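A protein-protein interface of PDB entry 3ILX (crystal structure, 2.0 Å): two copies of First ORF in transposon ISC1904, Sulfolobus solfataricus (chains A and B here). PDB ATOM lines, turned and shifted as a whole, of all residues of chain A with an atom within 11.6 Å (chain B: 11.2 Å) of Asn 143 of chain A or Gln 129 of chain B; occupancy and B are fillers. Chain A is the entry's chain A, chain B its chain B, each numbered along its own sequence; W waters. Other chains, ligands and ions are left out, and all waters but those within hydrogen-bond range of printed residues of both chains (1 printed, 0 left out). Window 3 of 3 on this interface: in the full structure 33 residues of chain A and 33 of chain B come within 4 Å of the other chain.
The side-chain carboxylate (OE2) of Glu 105 of chain A sits at hydrogen-bond distance from the side-chain hydroxyl (OG) of Ser 128 of chain B (2.6 Å). SG of Cys 137 of chain A is disulfide-bonded to SG of Cys 137 of chain B, 2.3 Å away. NZ of Lys 133 of chain B lies within hydrogen-bond range of O of Glu 140 of chain A (2.6 Å). The chain-end carboxylate (O) of Asn 143 of chain A lies within salt-bridge range of the side-chain amino group (NZ) of Lys 130 of chain B (3.0 Å). O of Asn 143 of chain A is in salt-bridge range of NZ of Lys 133 of chain B, 2.9 Å away.
The side-chain carboxylate of Glu 140 of chain A lies within salt-bridge range of the side-chain amino group of Lys 136 of chain A (3.5 Å). The backbone carbonyl oxygen (O) of Leu 123 of chain B is in hydrogen-bond range of the backbone NH (N) of Ser 128 of chain B (3.1 Å). OE1 of Gln 129 of chain B is in hydrogen-bond range of NZ of Lys 130 of chain B (3.2 Å). OE1 of Gln 129 of chain B sits at hydrogen-bond distance from NZ of Lys 133 of chain B (3.1 Å).
Among the printed residues, pairs that only touch across the chains: Glu 105 of chain A with Lys 130 of chain B (3.6 Å), Leu 108 of chain A with Phe 119 of chain B (3.1 Å), Leu 108 of chain A with Lys 122 of chain B (3.7 Å), Leu 108 of chain A with Leu 123 of chain B (3.8 Å), Leu 108 of chain A with Met 126 of chain B (3.7 Å), Val 109 of chain A with Lys 130 of chain B (3.9 Å), Leu 112 of chain A with Phe 119 of chain B (3.9 Å), Leu 112 of chain A with Val 134 of chain B (3.7 Å), Leu 141 of chain A with Lys 130 of chain B (3.2 Å), Leu 141 of chain A with Val 134 of chain B (3.8 Å) and Asn 143 of chain A with Gln 129 of chain B (3.7 Å).
Printed residues of chain B within 4 Å of Glu 105 of chain A: Ser 128 and Lys 130. Glu 106 of chain A touches none of the printed residues of chain B. Printed residues of chain B within 4 Å of Val 109 of chain A: Lys 130 (3.9 Å). No residue of chain B comes within 4 Å of Glu 139 of chain A. Asn 143 of chain A touches three residues of chain B. Printed residues of chain A within 4 Å of Lys 122 of chain B: Leu 108. Of the printed residues of chain A, Met 126 of chain B touches Leu 108. Ser 128 of chain B touches just one residue of chain A: Glu 105. Of the printed residues of chain A, Gln 129 of chain B touches Asn 143. Printed residues of chain A within 4 Å of Lys 130 of chain B: Glu 105, Val 109, Leu 141 and Asn 143. No residue of chain A comes within 4 Å of Glu 132 of chain B. The nearest residue of chain B that does not touch Asn 143 of chain A is Ser 128 of chain B (9.1 Å). The nearest residue of chain A that does not touch Gln 129 of chain B is Glu 105 of chain A (4.1 Å).
Printed residues of chain B that touch a printed residue of chain A: Phe 119, Lys 122, Leu 123, Met 126, Ser 128, Gln 129, Lys 130, Lys 133, Val 134 and Cys 137. Hydrophobic or aromatic side chains of chain B that line the printed part of chain A: Phe 119, Leu 123, Met 126 and Val 134. Printed residues of chain A that touch a printed residue of chain B: Glu 105, Leu 108, Val 109, Leu 112, Cys 137, Glu 140, Leu 141 and Asn 143. Among the printed residues, no Asp or Glu carboxylate lies within 4 Å of a Lys or Arg side-chain nitrogen of the other chain.
Cys 137 of chain B touches its own counterpart, Cys 137 of chain A. Positions printed for both chains: 134, 135, 136 and 137.
Water W1 lies within hydrogen-bond range of OXT of Asn 143 of chain A and NE2 of Gln 129 of chain B.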
ATOM      1  N   PRO A 104     -22.631  38.779 -29.781  1.00  0.00           N
ATOM      2  CA  PRO A 104     -21.904  38.792 -28.500  1.00  0.00           C
ATOM      3  C   PRO A 104     -22.138  37.514 -27.692  1.00  0.00           C
ATOM      4  O   PRO A 104     -23.221  36.906 -27.756  1.00  0.00           O
ATOM      5  CB  PRO A 104     -22.525  39.978 -27.752  1.00  0.00           C
ATOM      6  CG  PRO A 104     -23.110  40.837 -28.831  1.00  0.00           C
ATOM      7  CD  PRO A 104     -23.646  39.848 -29.816  1.00  0.00           C
ATOM      8  N   GLU A 105     -21.133  37.138 -26.914  1.00  0.00           N
ATOM      9  CA  GLU A 105     -21.179  35.928 -26.131  1.00  0.00           C
ATOM     10  C   GLU A 105     -22.400  35.931 -25.224  1.00  0.00           C
ATOM     11  O   GLU A 105     -23.120  34.936 -25.159  1.00  0.00           O
ATOM     12  CB  GLU A 105     -19.904  35.783 -25.299  1.00  0.00           C
ATOM     13  CG  GLU A 105     -19.995  34.641 -24.290  1.00  0.00           C
ATOM     14  CD  GLU A 105     -18.655  34.242 -23.731  1.00  0.00           C
ATOM     15  OE1 GLU A 105     -17.627  34.769 -24.194  1.00  0.00           O
ATOM     16  OE2 GLU A 105     -18.627  33.378 -22.841  1.00  0.00           O
ATOM     17  N   GLU A 106     -22.613  37.040 -24.529  1.00  0.00           N
ATOM     18  CA  GLU A 106     -23.730  37.190 -23.590  1.00  0.00           C
ATOM     19  C   GLU A 106     -25.071  36.903 -24.263  1.00  0.00           C
ATOM     20  O   GLU A 106     -25.975  36.370 -23.626  1.00  0.00           O
ATOM     21  CB  GLU A 106     -23.735  38.614 -23.002  1.00  0.00           C
ATOM     22  CG  GLU A 106     -24.866  38.901 -22.004  1.00  0.00           C
ATOM     23  CD  GLU A 106     -25.029  40.395 -21.659  1.00  0.00           C
ATOM     24  OE1 GLU A 106     -24.073  41.190 -21.840  1.00  0.00           O
ATOM     25  OE2 GLU A 106     -26.133  40.771 -21.202  1.00  0.00           O
ATOM     26  N   LEU A 108     -25.697  34.946 -26.968  1.00  0.00           N
ATOM     27  CA  LEU A 108     -25.858  33.527 -27.248  1.00  0.00           C
ATOM     28  C   LEU A 108     -26.201  32.715 -26.001  1.00  0.00           C
ATOM     29  O   LEU A 108     -27.010  31.780 -26.094  1.00  0.00           O
ATOM     30  CB  LEU A 108     -24.609  32.942 -27.835  1.00  0.00           C
ATOM     31  CG  LEU A 108     -24.167  33.350 -29.230  1.00  0.00           C
ATOM     32  CD1 LEU A 108     -22.723  32.954 -29.380  1.00  0.00           C
ATOM     33  CD2 LEU A 108     -25.045  32.661 -30.290  1.00  0.00           C
ATOM     34  N   VAL A 109     -25.567  33.067 -24.874  1.00  0.00           N
ATOM     35  CA  VAL A 109     -25.741  32.354 -23.610  1.00  0.00           C
ATOM     36  C   VAL A 109     -27.156  32.602 -23.103  1.00  0.00           C
ATOM     37  O   VAL A 109     -27.834  31.699 -22.592  1.00  0.00           O
ATOM     38  CB  VAL A 109     -24.675  32.812 -22.570  1.00  0.00           C
ATOM     39  CG1 VAL A 109     -24.985  32.342 -21.170  1.00  0.00           C
ATOM     40  CG2 VAL A 109     -23.246  32.341 -22.992  1.00  0.00           C
ATOM     41  N   GLU A 110     -27.592  33.845 -23.243  1.00  0.00           N
ATOM     42  CA  GLU A 110     -28.923  34.243 -22.860  1.00  0.00           C
ATOM     43  C   GLU A 110     -29.971  33.517 -23.696  1.00  0.00           C
ATOM     44  O   GLU A 110     -30.991  33.061 -23.162  1.00  0.00           O
ATOM     45  CB  GLU A 110     -29.062  35.739 -23.039  1.00  0.00           C
ATOM     46  CG  GLU A 110     -30.405  36.275 -22.689  1.00  0.00           C
ATOM     47  CD  GLU A 110     -30.580  37.717 -23.153  1.00  0.00           C
ATOM     48  OE1 GLU A 110     -29.571  38.462 -23.291  1.00  0.00           O
ATOM     49  OE2 GLU A 110     -31.736  38.095 -23.401  1.00  0.00           O
ATOM     50  N   LEU A 112     -29.547  30.619 -25.376  1.00  0.00           N
ATOM     51  CA  LEU A 112     -29.512  29.218 -24.956  1.00  0.00           C
ATOM     52  C   LEU A 112     -30.253  28.985 -23.619  1.00  0.00           C
ATOM     53  O   LEU A 112     -31.020  28.033 -23.501  1.00  0.00           O
ATOM     54  CB  LEU A 112     -28.092  28.675 -24.915  1.00  0.00           C
ATOM     55  CG  LEU A 112     -27.974  27.147 -24.815  1.00  0.00           C
ATOM     56  CD1 LEU A 112     -28.876  26.391 -25.810  1.00  0.00           C
ATOM     57  CD2 LEU A 112     -26.516  26.792 -25.055  1.00  0.00           C
ATOM     58  N   ALA A 113     -30.057  29.867 -22.651  1.00  0.00           N
ATOM     59  CA  ALA A 113     -30.766  29.750 -21.364  1.00  0.00           C
ATOM     60  C   ALA A 113     -32.297  29.819 -21.544  1.00  0.00           C
ATOM     61  O   ALA A 113     -33.066  29.087 -20.889  1.00  0.00           O
ATOM     62  CB  ALA A 113     -30.288  30.855 -20.391  1.00  0.00           C
ATOM     63  N   LEU A 116     -33.214  26.461 -23.148  1.00  0.00           N
ATOM     64  CA  LEU A 116     -33.084  25.392 -22.135  1.00  0.00           C
ATOM     65  C   LEU A 116     -34.253  25.389 -21.168  1.00  0.00           C
ATOM     66  O   LEU A 116     -34.805  24.328 -20.880  1.00  0.00           O
ATOM     67  CB  LEU A 116     -31.765  25.504 -21.355  1.00  0.00           C
ATOM     68  CG  LEU A 116     -30.544  25.130 -22.213  1.00  0.00           C
ATOM     69  CD1 LEU A 116     -29.270  25.525 -21.496  1.00  0.00           C
ATOM     70  CD2 LEU A 116     -30.531  23.663 -22.573  1.00  0.00           C
ATOM     71  N   VAL A 134     -31.096  18.835 -18.216  1.00  0.00           N
ATOM     72  CA  VAL A 134     -31.393  20.109 -18.871  1.00  0.00           C
ATOM     73  C   VAL A 134     -31.342  21.285 -17.864  1.00  0.00           C
ATOM     74  O   VAL A 134     -30.742  22.319 -18.157  1.00  0.00           O
ATOM     75  CB  VAL A 134     -32.736  20.055 -19.682  1.00  0.00           C
ATOM     76  CG1 VAL A 134     -33.021  21.399 -20.315  1.00  0.00           C
ATOM     77  CG2 VAL A 134     -32.636  18.992 -20.781  1.00  0.00           C
ATOM     78  N   LYS A 135     -31.917  21.081 -16.671  1.00  0.00           N
ATOM     79  CA  LYS A 135     -31.821  22.031 -15.571  1.00  0.00           C
ATOM     80  C   LYS A 135     -30.344  22.303 -15.191  1.00  0.00           C
ATOM     81  O   LYS A 135     -29.903  23.448 -15.082  1.00  0.00           O
ATOM     82  CB  LYS A 135     -32.582  21.459 -14.393  1.00  0.00           C
ATOM     83  CG  LYS A 135     -32.817  22.422 -13.263  1.00  0.00           C
ATOM     84  CD  LYS A 135     -33.095  21.644 -11.995  1.00  0.00           C
ATOM     85  CE  LYS A 135     -32.496  22.309 -10.772  1.00  0.00           C
ATOM     86  NZ  LYS A 135     -32.916  21.517  -9.569  1.00  0.00           N
ATOM     87  N   LYS A 136     -29.587  21.229 -15.014  1.00  0.00           N
ATOM     88  CA  LYS A 136     -28.183  21.306 -14.702  1.00  0.00           C
ATOM     89  C   LYS A 136     -27.400  22.105 -15.766  1.00  0.00           C
ATOM     90  O   LYS A 136     -26.488  22.878 -15.425  1.00  0.00           O
ATOM     91  CB  LYS A 136     -27.671  19.872 -14.540  1.00  0.00           C
ATOM     92  CG  LYS A 136     -26.242  19.642 -14.908  1.00  0.00           C
ATOM     93  CD  LYS A 136     -25.402  19.523 -13.683  1.00  0.00           C
ATOM     94  CE  LYS A 136     -23.990  19.888 -14.025  1.00  0.00           C
ATOM     95  NZ  LYS A 136     -23.312  20.204 -12.749  1.00  0.00           N
ATOM     96  N   CYS A 137     -27.747  21.929 -17.042  1.00  0.00           N
ATOM     97  CA  CYS A 137     -27.116  22.696 -18.132  1.00  0.00           C
ATOM     98  C   CYS A 137     -27.442  24.183 -18.050  1.00  0.00           C
ATOM     99  O   CYS A 137     -26.550  25.018 -18.178  1.00  0.00           O
ATOM    100  CB  CYS A 137     -27.536  22.180 -19.510  1.00  0.00           C
ATOM    101  SG  CYS A 137     -27.001  20.509 -19.892  1.00  0.00           S
ATOM    102  N   ALA A 138     -28.718  24.512 -17.854  1.00  0.00           N
ATOM    103  CA  ALA A 138     -29.124  25.911 -17.657  1.00  0.00           C
ATOM    104  C   ALA A 138     -28.371  26.544 -16.467  1.00  0.00           C
ATOM    105  O   ALA A 138     -27.855  27.657 -16.565  1.00  0.00           O
ATOM    106  CB  ALA A 138     -30.663  26.021 -17.509  1.00  0.00           C
ATOM    107  N   GLU A 139     -28.242  25.801 -15.375  1.00  0.00           N
ATOM    108  CA  GLU A 139     -27.459  26.266 -14.236  1.00  0.00           C
ATOM    109  C   GLU A 139     -25.966  26.539 -14.589  1.00  0.00           C
ATOM    110  O   GLU A 139     -25.418  27.616 -14.267  1.00  0.00           O
ATOM    111  CB  GLU A 139     -27.611  25.273 -13.069  1.00  0.00           C
ATOM    112  CG  GLU A 139     -26.708  25.530 -11.874  1.00  0.00           C
ATOM    113  CD  GLU A 139     -27.134  26.735 -11.007  1.00  0.00           C
ATOM    114  OE1 GLU A 139     -28.280  27.238 -11.150  1.00  0.00           O
ATOM    115  OE2 GLU A 139     -26.299  27.180 -10.176  1.00  0.00           O
ATOM    116  N   GLU A 140     -25.324  25.579 -15.255  1.00  0.00           N
ATOM    117  CA  GLU A 140     -23.926  25.738 -15.665  1.00  0.00           C
ATOM    118  C   GLU A 140     -23.764  27.025 -16.494  1.00  0.00           C
ATOM    119  O   GLU A 140     -22.787  27.756 -16.313  1.00  0.00           O
ATOM    120  CB  GLU A 140     -23.413  24.515 -16.454  1.00  0.00           C
ATOM    121  CG  GLU A 140     -23.096  23.266 -15.617  1.00  0.00           C
ATOM    122  CD  GLU A 140     -21.978  23.506 -14.633  1.00  0.00           C
ATOM    123  OE1 GLU A 140     -20.834  23.770 -15.060  1.00  0.00           O
ATOM    124  OE2 GLU A 140     -22.246  23.459 -13.417  1.00  0.00           O
ATOM    125  N   LEU A 141     -24.731  27.313 -17.372  1.00  0.00           N
ATOM    126  CA  LEU A 141     -24.659  28.496 -18.240  1.00  0.00           C
ATOM    127  C   LEU A 141     -24.905  29.797 -17.513  1.00  0.00           C
ATOM    128  O   LEU A 141     -24.453  30.841 -17.980  1.00  0.00           O
ATOM    129  CB  LEU A 141     -25.611  28.407 -19.441  1.00  0.00           C
ATOM    130  CG  LEU A 141     -25.274  27.415 -20.538  1.00  0.00           C
ATOM    131  CD1 LEU A 141     -26.288  27.586 -21.672  1.00  0.00           C
ATOM    132  CD2 LEU A 141     -23.845  27.605 -21.056  1.00  0.00           C
ATOM    133  N   LYS A 142     -25.659  29.745 -16.416  1.00  0.00           N
ATOM    134  CA  LYS A 142     -25.827  30.901 -15.544  1.00  0.00           C
ATOM    135  C   LYS A 142     -24.618  31.187 -14.619  1.00  0.00           C
ATOM    136  O   LYS A 142     -24.594  32.197 -13.938  1.00  0.00           O
ATOM    137  CB  LYS A 142     -27.075  30.730 -14.686  1.00  0.00           C
ATOM    138  CG  LYS A 142     -28.345  31.157 -15.372  1.00  0.00           C
ATOM    139  CD  LYS A 142     -29.375  31.483 -14.305  1.00  0.00           C
ATOM    140  CE  LYS A 142     -30.714  31.803 -14.922  1.00  0.00           C
ATOM    141  NZ  LYS A 142     -31.757  31.960 -13.848  1.00  0.00           N
ATOM    142  N   ASN A 143     -23.645  30.283 -14.605  1.00  0.00           N
ATOM    143  CA  ASN A 143     -22.446  30.431 -13.812  1.00  0.00           C
ATOM    144  C   ASN A 143     -21.295  31.041 -14.596  1.00  0.00           C
ATOM    145  O   ASN A 143     -21.079  30.673 -15.755  1.00  0.00           O
ATOM    146  CB  ASN A 143     -22.014  29.083 -13.254  1.00  0.00           C
ATOM    147  CG  ASN A 143     -22.675  28.768 -11.949  1.00  0.00           C
ATOM    148  OD1 ASN A 143     -22.042  28.846 -10.889  1.00  0.00           O
ATOM    149  ND2 ASN A 143     -23.967  28.443 -11.993  1.00  0.00           N
ATOM    150  OXT ASN A 143     -20.569  31.894 -14.065  1.00  0.00           O
ATOM    151  N   PHE B 119     -25.107  25.734 -31.082  1.00  0.00           N
ATOM    152  CA  PHE B 119     -24.546  26.754 -30.172  1.00  0.00           C
ATOM    153  C   PHE B 119     -23.059  26.537 -29.839  1.00  0.00           C
ATOM    154  O   PHE B 119     -22.276  27.490 -29.828  1.00  0.00           O
ATOM    155  CB  PHE B 119     -25.388  26.858 -28.904  1.00  0.00           C
ATOM    156  CG  PHE B 119     -26.520  27.823 -29.038  1.00  0.00           C
ATOM    157  CD1 PHE B 119     -26.414  29.117 -28.509  1.00  0.00           C
ATOM    158  CD2 PHE B 119     -27.669  27.474 -29.773  1.00  0.00           C
ATOM    159  CE1 PHE B 119     -27.472  30.037 -28.666  1.00  0.00           C
ATOM    160  CE2 PHE B 119     -28.728  28.391 -29.930  1.00  0.00           C
ATOM    161  CZ  PHE B 119     -28.626  29.677 -29.382  1.00  0.00           C
ATOM    162  N   SER B 120     -22.659  25.282 -29.595  1.00  0.00           N
ATOM    163  CA  SER B 120     -21.234  25.047 -29.303  1.00  0.00           C
ATOM    164  C   SER B 120     -20.373  25.486 -30.470  1.00  0.00           C
ATOM    165  O   SER B 120     -19.287  26.017 -30.263  1.00  0.00           O
ATOM    166  CB  SER B 120     -20.942  23.600 -28.887  1.00  0.00           C
ATOM    167  OG  SER B 120     -21.312  22.684 -29.892  1.00  0.00           O
ATOM    168  N   LYS B 122     -21.118  27.963 -32.538  1.00  0.00           N
ATOM    169  CA  LYS B 122     -21.136  29.426 -32.478  1.00  0.00           C
ATOM    170  C   LYS B 122     -20.202  29.942 -31.351  1.00  0.00           C
ATOM    171  O   LYS B 122     -19.533  30.955 -31.512  1.00  0.00           O
ATOM    172  CB  LYS B 122     -22.564  29.975 -32.302  1.00  0.00           C
ATOM    173  CG  LYS B 122     -23.604  29.636 -33.405  1.00  0.00           C
ATOM    174  CD  LYS B 122     -24.990  30.055 -32.898  1.00  0.00           C
ATOM    175  CE  LYS B 122     -26.181  29.317 -33.536  1.00  0.00           C
ATOM    176  NZ  LYS B 122     -26.630  30.001 -34.761  1.00  0.00           N
ATOM    177  N   LEU B 123     -20.142  29.218 -30.234  1.00  0.00           N
ATOM    178  CA  LEU B 123     -19.312  29.614 -29.096  1.00  0.00           C
ATOM    179  C   LEU B 123     -17.844  29.250 -29.291  1.00  0.00           C
ATOM    180  O   LEU B 123     -16.958  29.849 -28.681  1.00  0.00           O
ATOM    181  CB  LEU B 123     -19.821  28.953 -27.823  1.00  0.00           C
ATOM    182  CG  LEU B 123     -21.181  29.438 -27.327  1.00  0.00           C
ATOM    183  CD1 LEU B 123     -21.753  28.426 -26.348  1.00  0.00           C
ATOM    184  CD2 LEU B 123     -21.065  30.790 -26.673  1.00  0.00           C
ATOM    185  N   HIS B 124     -17.598  28.238 -30.113  1.00  0.00           N
ATOM    186  CA  HIS B 124     -16.253  27.718 -30.264  1.00  0.00           C
ATOM    187  C   HIS B 124     -15.459  28.690 -31.113  1.00  0.00           C
ATOM    188  O   HIS B 124     -14.301  28.974 -30.814  1.00  0.00           O
ATOM    189  CB  HIS B 124     -16.245  26.329 -30.907  1.00  0.00           C
ATOM    190  CG  HIS B 124     -14.868  25.750 -31.064  1.00  0.00           C
ATOM    191  ND1 HIS B 124     -14.098  25.350 -29.988  1.00  0.00           N
ATOM    192  CD2 HIS B 124     -14.112  25.536 -32.166  1.00  0.00           C
ATOM    193  CE1 HIS B 124     -12.937  24.897 -30.423  1.00  0.00           C
ATOM    194  NE2 HIS B 124     -12.920  24.998 -31.741  1.00  0.00           N
ATOM    195  N   GLY B 125     -16.108  29.201 -32.160  1.00  0.00           N
ATOM    196  CA  GLY B 125     -15.490  30.136 -33.093  1.00  0.00           C
ATOM    197  C   GLY B 125     -14.833  31.267 -32.330  1.00  0.00           C
ATOM    198  O   GLY B 125     -13.684  31.626 -32.604  1.00  0.00           O
ATOM    199  N   MET B 126     -15.550  31.799 -31.343  1.00  0.00           N
ATOM    200  CA  MET B 126     -15.039  32.907 -30.528  1.00  0.00           C
ATOM    201  C   MET B 126     -14.101  32.468 -29.397  1.00  0.00           C
ATOM    202  O   MET B 126     -13.356  33.288 -28.870  1.00  0.00           O
ATOM    203  CB  MET B 126     -16.198  33.739 -29.964  1.00  0.00           C
ATOM    204  CG  MET B 126     -17.208  32.949 -29.160  1.00  0.00           C
ATOM    205  SD  MET B 126     -18.802  34.006 -28.828  1.00  0.00           S
ATOM    206  CE  MET B 126     -19.436  34.192 -30.668  1.00  0.00           C
ATOM    207  N   ARG B 127     -14.132  31.182 -29.051  1.00  0.00           N
ATOM    208  CA  ARG B 127     -13.388  30.627 -27.908  1.00  0.00           C
ATOM    209  C   ARG B 127     -13.895  31.181 -26.568  1.00  0.00           C
ATOM    210  O   ARG B 127     -13.147  31.759 -25.775  1.00  0.00           O
ATOM    211  CB  ARG B 127     -11.864  30.785 -28.070  1.00  0.00           C
ATOM    212  CG  ARG B 127     -11.290  29.944 -29.182  1.00  0.00           C
ATOM    213  CD  ARG B 127      -9.783  29.888 -29.130  1.00  0.00           C
ATOM    214  NE  ARG B 127      -9.120  31.189 -29.273  1.00  0.00           N
ATOM    215  CZ  ARG B 127      -9.194  31.984 -30.347  1.00  0.00           C
ATOM    216  NH1 ARG B 127      -9.943  31.650 -31.397  1.00  0.00           N
ATOM    217  NH2 ARG B 127      -8.526  33.137 -30.365  1.00  0.00           N
ATOM    218  N   SER B 128     -15.190  30.985 -26.338  1.00  0.00           N
ATOM    219  CA  SER B 128     -15.868  31.397 -25.115  1.00  0.00           C
ATOM    220  C   SER B 128     -15.636  30.368 -23.990  1.00  0.00           C
ATOM    221  O   SER B 128     -15.606  29.172 -24.273  1.00  0.00           O
ATOM    222  CB  SER B 128     -17.361  31.547 -25.446  1.00  0.00           C
ATOM    223  OG  SER B 128     -18.209  31.296 -24.337  1.00  0.00           O
ATOM    224  N   GLN B 129     -15.483  30.824 -22.735  1.00  0.00           N
ATOM    225  CA  GLN B 129     -15.386  29.926 -21.557  1.00  0.00           C
ATOM    226  C   GLN B 129     -16.459  28.849 -21.598  1.00  0.00           C
ATOM    227  O   GLN B 129     -16.283  27.777 -21.038  1.00  0.00           O
ATOM    228  CB  GLN B 129     -15.572  30.710 -20.240  1.00  0.00           C
ATOM    229  CG  GLN B 129     -15.943  29.817 -19.012  1.00  0.00           C
ATOM    230  CD  GLN B 129     -16.990  30.427 -18.059  1.00  0.00           C
ATOM    231  OE1 GLN B 129     -18.072  29.854 -17.823  1.00  0.00           O
ATOM    232  NE2 GLN B 129     -16.659  31.579 -17.495  1.00  0.00           N
ATOM    233  N   LYS B 130     -17.552  29.161 -22.297  1.00  0.00           N
ATOM    234  CA  LYS B 130     -18.799  28.429 -22.300  1.00  0.00           C
ATOM    235  C   LYS B 130     -18.867  27.246 -23.288  1.00  0.00           C
ATOM    236  O   LYS B 130     -19.768  26.410 -23.202  1.00  0.00           O
ATOM    237  CB  LYS B 130     -19.924  29.433 -22.582  1.00  0.00           C
ATOM    238  CG  LYS B 130     -20.150  30.452 -21.451  1.00  0.00           C
ATOM    239  CD  LYS B 130     -20.706  29.731 -20.208  1.00  0.00           C
ATOM    240  CE  LYS B 130     -21.518  30.644 -19.289  1.00  0.00           C
ATOM    241  NZ  LYS B 130     -20.661  31.579 -18.538  1.00  0.00           N
ATOM    242  N   TYR B 131     -17.911  27.174 -24.213  1.00  0.00           N
ATOM    243  CA  TYR B 131     -17.886  26.122 -25.211  1.00  0.00           C
ATOM    244  C   TYR B 131     -17.970  24.727 -24.579  1.00  0.00           C
ATOM    245  O   TYR B 131     -18.844  23.932 -24.922  1.00  0.00           O
ATOM    246  CB  TYR B 131     -16.630  26.262 -26.085  1.00  0.00           C
ATOM    247  CG  TYR B 131     -16.385  25.073 -26.987  1.00  0.00           C
ATOM    248  CD1 TYR B 131     -17.261  24.771 -28.025  1.00  0.00           C
ATOM    249  CD2 TYR B 131     -15.286  24.239 -26.789  1.00  0.00           C
ATOM    250  CE1 TYR B 131     -17.043  23.659 -28.863  1.00  0.00           C
ATOM    251  CE2 TYR B 131     -15.053  23.137 -27.617  1.00  0.00           C
ATOM    252  CZ  TYR B 131     -15.935  22.847 -28.647  1.00  0.00           C
ATOM    253  OH  TYR B 131     -15.711  21.755 -29.472  1.00  0.00           O
ATOM    254  N   GLU B 132     -17.093  24.457 -23.621  1.00  0.00           N
ATOM    255  CA  GLU B 132     -17.016  23.148 -22.984  1.00  0.00           C
ATOM    256  C   GLU B 132     -18.310  22.758 -22.249  1.00  0.00           C
ATOM    257  O   GLU B 132     -18.752  21.611 -22.345  1.00  0.00           O
ATOM    258  CB  GLU B 132     -15.830  23.109 -22.031  1.00  0.00           C
ATOM    259  CG  GLU B 132     -14.472  23.213 -22.722  1.00  0.00           C
ATOM    260  CD  GLU B 132     -14.066  21.963 -23.518  1.00  0.00           C
ATOM    261  OE1 GLU B 132     -14.712  20.901 -23.387  1.00  0.00           O
ATOM    262  OE2 GLU B 132     -13.071  22.043 -24.284  1.00  0.00           O
ATOM    263  N   LYS B 133     -18.925  23.704 -21.547  1.00  0.00           N
ATOM    264  CA  LYS B 133     -20.183  23.392 -20.847  1.00  0.00           C
ATOM    265  C   LYS B 133     -21.251  22.950 -21.836  1.00  0.00           C
ATOM    266  O   LYS B 133     -21.989  21.993 -21.598  1.00  0.00           O
ATOM    267  CB  LYS B 133     -20.686  24.587 -20.053  1.00  0.00           C
ATOM    268  CG  LYS B 133     -19.775  24.988 -18.901  1.00  0.00           C
ATOM    269  CD  LYS B 133     -20.156  26.406 -18.435  1.00  0.00           C
ATOM    270  CE  LYS B 133     -19.580  26.737 -17.065  1.00  0.00           C
ATOM    271  NZ  LYS B 133     -20.199  27.970 -16.466  1.00  0.00           N
ATOM    272  N   VAL B 134     -21.347  23.667 -22.944  1.00  0.00           N
ATOM    273  CA  VAL B 134     -22.360  23.372 -23.950  1.00  0.00           C
ATOM    274  C   VAL B 134     -22.054  22.040 -24.636  1.00  0.00           C
ATOM    275  O   VAL B 134     -22.959  21.234 -24.893  1.00  0.00           O
ATOM    276  CB  VAL B 134     -22.502  24.524 -24.976  1.00  0.00           C
ATOM    277  CG1 VAL B 134     -23.448  24.126 -26.076  1.00  0.00           C
ATOM    278  CG2 VAL B 134     -23.039  25.759 -24.273  1.00  0.00           C
ATOM    279  N   LYS B 135     -20.770  21.806 -24.895  1.00  0.00           N
ATOM    280  CA  LYS B 135     -20.321  20.556 -25.471  1.00  0.00           C
ATOM    281  C   LYS B 135     -20.682  19.399 -24.516  1.00  0.00           C
ATOM    282  O   LYS B 135     -21.190  18.367 -24.954  1.00  0.00           O
ATOM    283  CB  LYS B 135     -18.798  20.625 -25.708  1.00  0.00           C
ATOM    284  CG  LYS B 135     -18.320  19.817 -26.860  1.00  0.00           C
ATOM    285  CD  LYS B 135     -16.782  19.770 -26.882  1.00  0.00           C
ATOM    286  CE  LYS B 135     -16.302  18.500 -27.569  1.00  0.00           C
ATOM    287  NZ  LYS B 135     -15.077  17.959 -26.925  1.00  0.00           N
ATOM    288  N   LYS B 136     -20.442  19.581 -23.211  1.00  0.00           N
ATOM    289  CA  LYS B 136     -20.719  18.528 -22.225  1.00  0.00           C
ATOM    290  C   LYS B 136     -22.220  18.264 -22.129  1.00  0.00           C
ATOM    291  O   LYS B 136     -22.655  17.112 -22.050  1.00  0.00           O
ATOM    292  CB  LYS B 136     -20.193  18.908 -20.846  1.00  0.00           C
ATOM    293  CG  LYS B 136     -20.625  17.931 -19.765  1.00  0.00           C
ATOM    294  CD  LYS B 136     -20.551  18.524 -18.393  1.00  0.00           C
ATOM    295  CE  LYS B 136     -19.118  18.647 -17.929  1.00  0.00           C
ATOM    296  NZ  LYS B 136     -19.051  18.275 -16.477  1.00  0.00           N
ATOM    297  N   CYS B 137     -22.984  19.336 -22.135  1.00  0.00           N
ATOM    298  CA  CYS B 137     -24.406  19.245 -22.137  1.00  0.00           C
ATOM    299  C   CYS B 137     -24.948  18.371 -23.282  1.00  0.00           C
ATOM    300  O   CYS B 137     -25.827  17.534 -23.062  1.00  0.00           O
ATOM    301  CB  CYS B 137     -24.966  20.636 -22.263  1.00  0.00           C
ATOM    302  SG  CYS B 137     -26.680  20.588 -22.162  1.00  0.00           S
HETATM  303  O   HOH W   1     -18.422  31.854 -15.145  1.00  0.00           O
